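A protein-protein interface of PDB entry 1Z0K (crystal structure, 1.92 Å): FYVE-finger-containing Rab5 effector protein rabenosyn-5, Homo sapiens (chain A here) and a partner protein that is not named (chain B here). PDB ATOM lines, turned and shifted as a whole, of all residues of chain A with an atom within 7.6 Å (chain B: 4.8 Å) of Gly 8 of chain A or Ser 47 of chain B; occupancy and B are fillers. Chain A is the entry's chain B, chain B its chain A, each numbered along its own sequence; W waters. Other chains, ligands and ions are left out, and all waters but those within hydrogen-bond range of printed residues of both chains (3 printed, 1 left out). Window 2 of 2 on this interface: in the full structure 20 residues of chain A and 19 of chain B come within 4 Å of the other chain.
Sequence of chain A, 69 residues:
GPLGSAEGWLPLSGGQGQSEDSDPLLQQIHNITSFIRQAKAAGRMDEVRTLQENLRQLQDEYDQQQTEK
NZ of Lys 58 of chain B lies within salt-bridge range of OD2 of Asp 46 of chain A (3.7 Å).
The backbone carbonyl oxygen of Ser 47 of chain B is in hydrogen-bond range of the backbone NH of Trp 9 of chain A.
The side-chain amino group of Lys 58 of chain B lies within salt-bridge range of the side-chain carboxylate of Glu 47 of chain A (2.5 Å).
NH1 of Arg 44 of chain A lies within salt-bridge range of OE1 of Glu 47 of chain A, 3.1 Å away.
Among the printed residues, merely in contact across the chains: Gly 8 of chain A with Ile 29 of chain B (3.6 Å), Gly 8 of chain A with Ser 47 of chain B (3.1 Å), Trp 9 of chain A with Ile 29 of chain B (3.8 Å), Trp 9 of chain A with Phe 45 of chain B (3.8 Å), Trp 9 of chain A with Gly 46 of chain B (3.4 Å), Leu 10 of chain A with Phe 45 of chain B (3.2 Å), Pro 11 of chain A with Phe 45 of chain B (3.1 Å), Glu 47 of chain A with Phe 45 of chain B (3.9 Å) and Glu 47 of chain A with Ser 47 of chain B (3.5 Å).
Of the printed residues of chain B, Gly 8 of chain A touches Ile 29 and Ser 47.
Ser 47 of chain B touches just these residues of chain A: Gly 8 (3.1 Å), Trp 9 (2.8 Å) and Glu 47 (3.5 Å).
Printed residues of chain B within 4 Å of Trp 9 of chain A: Ile 29, Phe 45, Gly 46 and Ser 47.
Of the printed residues of chain A, Ile 29 of chain B touches Gly 8 and Trp 9.
Hydrophobic or aromatic side chains of chain A that line the printed part of chain B: Trp 9, Leu 10 and Pro 11.
Hydrophobic or aromatic side chains of chain B within 4 Å of the printed part of chain A: Ile 29 and Phe 45.
Among the printed residues, 12 pairs touch across the chains.
Water W1 lies within hydrogen-bond range of NZ of Lys 48 of chain B, O of Ile 49 of chain B and N of Glu 7 of chain A.
Water W3 lies within hydrogen-bond range of O of Ile 29 of chain B, NZ of Lys 48 of chain B, N of Gly 8 of chain A and OE1 of Glu 7 of chain A.
Water W2 bridges O of Phe 45 of chain B and O of Pro 11 of chain A.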
ATOM      1  N   GLU A   7     -21.789   7.844   2.744  1.00  0.00           N
ATOM      2  CA  GLU A   7     -23.203   7.522   2.372  1.00  0.00           C
ATOM      3  C   GLU A   7     -23.277   6.962   0.943  1.00  0.00           C
ATOM      4  O   GLU A   7     -23.238   7.712  -0.039  1.00  0.00           O
ATOM      5  CB  GLU A   7     -24.103   8.755   2.561  1.00  0.00           C
ATOM      6  CG  GLU A   7     -25.592   8.547   2.248  1.00  0.00           C
ATOM      7  CD  GLU A   7     -26.239   7.402   3.025  1.00  0.00           C
ATOM      8  OE1 GLU A   7     -25.837   7.126   4.181  1.00  0.00           O
ATOM      9  OE2 GLU A   7     -27.174   6.779   2.470  1.00  0.00           O
ATOM     10  N   GLY A   8     -23.393   5.639   0.857  1.00  0.00           N
ATOM     11  CA  GLY A   8     -23.169   4.893  -0.378  1.00  0.00           C
ATOM     12  C   GLY A   8     -24.162   5.087  -1.505  1.00  0.00           C
ATOM     13  O   GLY A   8     -25.156   5.800  -1.367  1.00  0.00           O
ATOM     14  N   TRP A   9     -23.881   4.431  -2.627  1.00  0.00           N
ATOM     15  CA  TRP A   9     -24.699   4.551  -3.824  1.00  0.00           C
ATOM     16  C   TRP A   9     -25.005   3.171  -4.388  1.00  0.00           C
ATOM     17  O   TRP A   9     -24.132   2.304  -4.449  1.00  0.00           O
ATOM     18  CB  TRP A   9     -23.989   5.425  -4.869  1.00  0.00           C
ATOM     19  CG  TRP A   9     -24.760   5.601  -6.146  1.00  0.00           C
ATOM     20  CD1 TRP A   9     -25.873   6.365  -6.336  1.00  0.00           C
ATOM     21  CD2 TRP A   9     -24.465   5.001  -7.409  1.00  0.00           C
ATOM     22  NE1 TRP A   9     -26.296   6.272  -7.642  1.00  0.00           N
ATOM     23  CE2 TRP A   9     -25.447   5.442  -8.321  1.00  0.00           C
ATOM     24  CE3 TRP A   9     -23.466   4.127  -7.860  1.00  0.00           C
ATOM     25  CZ2 TRP A   9     -25.458   5.042  -9.658  1.00  0.00           C
ATOM     26  CZ3 TRP A   9     -23.478   3.732  -9.186  1.00  0.00           C
ATOM     27  CH2 TRP A   9     -24.468   4.188 -10.070  1.00  0.00           C
ATOM     28  N   LEU A  10     -26.253   2.980  -4.801  1.00  0.00           N
ATOM     29  CA  LEU A  10     -26.721   1.693  -5.282  1.00  0.00           C
ATOM     30  C   LEU A  10     -27.797   1.911  -6.350  1.00  0.00           C
ATOM     31  O   LEU A  10     -28.947   2.208  -6.025  1.00  0.00           O
ATOM     32  CB  LEU A  10     -27.242   0.869  -4.100  1.00  0.00           C
ATOM     33  CG  LEU A  10     -27.746  -0.563  -4.225  1.00  0.00           C
ATOM     34  CD1 LEU A  10     -26.807  -1.457  -4.988  1.00  0.00           C
ATOM     35  CD2 LEU A  10     -27.957  -1.101  -2.826  1.00  0.00           C
ATOM     36  N   PRO A  11     -27.415   1.783  -7.633  1.00  0.00           N
ATOM     37  CA  PRO A  11     -28.308   2.052  -8.756  1.00  0.00           C
ATOM     38  C   PRO A  11     -29.404   1.008  -8.894  1.00  0.00           C
ATOM     39  O   PRO A  11     -29.167  -0.174  -8.621  1.00  0.00           O
ATOM     40  CB  PRO A  11     -27.373   1.983  -9.963  1.00  0.00           C
ATOM     41  CG  PRO A  11     -26.288   1.062  -9.533  1.00  0.00           C
ATOM     42  CD  PRO A  11     -26.075   1.379  -8.089  1.00  0.00           C
ATOM     43  N   ARG A  44     -21.852  11.336 -10.344  1.00  0.00           N
ATOM     44  CA  ARG A  44     -20.841  10.499  -9.704  1.00  0.00           C
ATOM     45  C   ARG A  44     -19.833   9.997 -10.730  1.00  0.00           C
ATOM     46  O   ARG A  44     -19.895   8.842 -11.164  1.00  0.00           O
ATOM     47  CB  ARG A  44     -21.506   9.320  -8.994  1.00  0.00           C
ATOM     48  CG  ARG A  44     -22.417   9.715  -7.851  1.00  0.00           C
ATOM     49  CD  ARG A  44     -22.933   8.494  -7.124  1.00  0.00           C
ATOM     50  NE  ARG A  44     -23.294   8.796  -5.739  1.00  0.00           N
ATOM     51  CZ  ARG A  44     -22.518   8.552  -4.687  1.00  0.00           C
ATOM     52  NH1 ARG A  44     -21.325   7.992  -4.844  1.00  0.00           N
ATOM     53  NH2 ARG A  44     -22.941   8.857  -3.470  1.00  0.00           N
ATOM     54  N   ASP A  46     -16.668   9.176 -10.659  1.00  0.00           N
ATOM     55  CA  ASP A  46     -15.876   8.003 -10.293  1.00  0.00           C
ATOM     56  C   ASP A  46     -16.610   6.718 -10.700  1.00  0.00           C
ATOM     57  O   ASP A  46     -16.027   5.835 -11.332  1.00  0.00           O
ATOM     58  CB  ASP A  46     -15.569   7.989  -8.786  1.00  0.00           C
ATOM     59  CG  ASP A  46     -14.361   8.847  -8.414  1.00  0.00           C
ATOM     60  OD1 ASP A  46     -13.763   9.493  -9.310  1.00  0.00           O
ATOM     61  OD2 ASP A  46     -14.001   8.863  -7.214  1.00  0.00           O
ATOM     62  N   GLU A  47     -17.890   6.643 -10.352  1.00  0.00           N
ATOM     63  CA  GLU A  47     -18.730   5.483 -10.671  1.00  0.00           C
ATOM     64  C   GLU A  47     -19.016   5.360 -12.167  1.00  0.00           C
ATOM     65  O   GLU A  47     -18.999   4.253 -12.715  1.00  0.00           O
ATOM     66  CB  GLU A  47     -20.032   5.531  -9.872  1.00  0.00           C
ATOM     67  CG  GLU A  47     -19.884   5.076  -8.425  1.00  0.00           C
ATOM     68  CD  GLU A  47     -19.208   6.109  -7.552  1.00  0.00           C
ATOM     69  OE1 GLU A  47     -19.764   7.207  -7.369  1.00  0.00           O
ATOM     70  OE2 GLU A  47     -18.114   5.817  -7.042  1.00  0.00           O
ATOM     71  N   ILE B  29     -25.812  -0.738   2.236  1.00  0.00           N
ATOM     72  CA  ILE B  29     -25.773   0.614   1.690  1.00  0.00           C
ATOM     73  C   ILE B  29     -26.991   1.438   2.091  1.00  0.00           C
ATOM     74  O   ILE B  29     -26.857   2.582   2.515  1.00  0.00           O
ATOM     75  CB  ILE B  29     -25.560   0.599   0.152  1.00  0.00           C
ATOM     76  CG1 ILE B  29     -24.169   0.034  -0.168  1.00  0.00           C
ATOM     77  CG2 ILE B  29     -25.750   2.006  -0.454  1.00  0.00           C
ATOM     78  CD1 ILE B  29     -23.920  -0.230  -1.637  1.00  0.00           C
ATOM     79  N   PHE B  45     -24.254  -3.550  -8.866  1.00  0.00           N
ATOM     80  CA  PHE B  45     -23.153  -2.712  -8.395  1.00  0.00           C
ATOM     81  C   PHE B  45     -23.552  -1.811  -7.240  1.00  0.00           C
ATOM     82  O   PHE B  45     -24.623  -1.219  -7.247  1.00  0.00           O
ATOM     83  CB  PHE B  45     -22.619  -1.828  -9.528  1.00  0.00           C
ATOM     84  CG  PHE B  45     -21.475  -0.949  -9.111  1.00  0.00           C
ATOM     85  CD1 PHE B  45     -20.197  -1.479  -8.967  1.00  0.00           C
ATOM     86  CD2 PHE B  45     -21.676   0.406  -8.846  1.00  0.00           C
ATOM     87  CE1 PHE B  45     -19.131  -0.678  -8.582  1.00  0.00           C
ATOM     88  CE2 PHE B  45     -20.615   1.219  -8.461  1.00  0.00           C
ATOM     89  CZ  PHE B  45     -19.340   0.681  -8.327  1.00  0.00           C
ATOM     90  N   GLY B  46     -22.662  -1.690  -6.265  1.00  0.00           N
ATOM     91  CA  GLY B  46     -22.836  -0.744  -5.176  1.00  0.00           C
ATOM     92  C   GLY B  46     -21.495  -0.159  -4.783  1.00  0.00           C
ATOM     93  O   GLY B  46     -20.458  -0.796  -4.923  1.00  0.00           O
ATOM     94  N   SER B  47     -21.520   1.069  -4.294  1.00  0.00           N
ATOM     95  CA  SER B  47     -20.311   1.723  -3.854  1.00  0.00           C
ATOM     96  C   SER B  47     -20.557   2.319  -2.468  1.00  0.00           C
ATOM     97  O   SER B  47     -21.591   2.946  -2.244  1.00  0.00           O
ATOM     98  CB  SER B  47     -19.925   2.781  -4.895  1.00  0.00           C
ATOM     99  OG  SER B  47     -19.203   3.843  -4.333  1.00  0.00           O
ATOM    100  N   LYS B  48     -19.639   2.080  -1.528  1.00  0.00           N
ATOM    101  CA  LYS B  48     -19.742   2.668  -0.183  1.00  0.00           C
ATOM    102  C   LYS B  48     -18.371   2.843   0.468  1.00  0.00           C
ATOM    103  O   LYS B  48     -17.518   1.973   0.370  1.00  0.00           O
ATOM    104  CB  LYS B  48     -20.655   1.825   0.725  1.00  0.00           C
ATOM    105  CG  LYS B  48     -20.821   2.356   2.141  1.00  0.00           C
ATOM    106  CD  LYS B  48     -21.921   1.591   2.879  1.00  0.00           C
ATOM    107  CE  LYS B  48     -21.970   1.950   4.351  1.00  0.00           C
ATOM    108  NZ  LYS B  48     -22.564   3.289   4.555  1.00  0.00           N
ATOM    109  N   ILE B  49     -18.181   3.969   1.149  1.00  0.00           N
ATOM    110  CA  ILE B  49     -16.927   4.253   1.847  1.00  0.00           C
ATOM    111  C   ILE B  49     -17.093   3.977   3.337  1.00  0.00           C
ATOM    112  O   ILE B  49     -18.031   4.456   3.955  1.00  0.00           O
ATOM    113  CB  ILE B  49     -16.461   5.719   1.607  1.00  0.00           C
ATOM    114  CG1 ILE B  49     -16.174   5.938   0.117  1.00  0.00           C
ATOM    115  CG2 ILE B  49     -15.210   6.043   2.444  1.00  0.00           C
ATOM    116  CD1 ILE B  49     -16.146   7.405  -0.308  1.00  0.00           C
ATOM    117  N   LYS B  58     -12.936   2.932   0.164  1.00  0.00           N
ATOM    118  CA  LYS B  58     -14.044   2.871  -0.762  1.00  0.00           C
ATOM    119  C   LYS B  58     -14.148   1.444  -1.269  1.00  0.00           C
ATOM    120  O   LYS B  58     -13.174   0.872  -1.765  1.00  0.00           O
ATOM    121  CB  LYS B  58     -13.853   3.849  -1.927  1.00  0.00           C
ATOM    122  CG  LYS B  58     -15.012   3.881  -2.908  1.00  0.00           C
ATOM    123  CD  LYS B  58     -14.953   5.110  -3.789  1.00  0.00           C
ATOM    124  CE  LYS B  58     -15.831   4.939  -5.011  1.00  0.00           C
ATOM    125  NZ  LYS B  58     -16.092   6.256  -5.671  1.00  0.00           N
ATOM    126  N   LEU B  59     -15.337   0.873  -1.109  1.00  0.00           N
ATOM    127  CA  LEU B  59     -15.633  -0.452  -1.616  1.00  0.00           C
ATOM    128  C   LEU B  59     -16.411  -0.338  -2.911  1.00  0.00           C
ATOM    129  O   LEU B  59     -17.427   0.349  -2.987  1.00  0.00           O
ATOM    130  CB  LEU B  59     -16.413  -1.283  -0.584  1.00  0.00           C
ATOM    131  CG  LEU B  59     -15.778  -1.374   0.809  1.00  0.00           C
ATOM    132  CD1 LEU B  59     -16.720  -2.063   1.802  1.00  0.00           C
ATOM    133  CD2 LEU B  59     -14.409  -2.064   0.759  1.00  0.00           C
HETATM  134  O   HOH W   1     -20.896   5.341   4.150  1.00  0.00           O
HETATM  135  O   HOH W   2     -26.769  -2.178  -8.672  1.00  0.00           O
HETATM  136  O   HOH W   3     -24.688   4.188   2.918  1.00  0.00           O
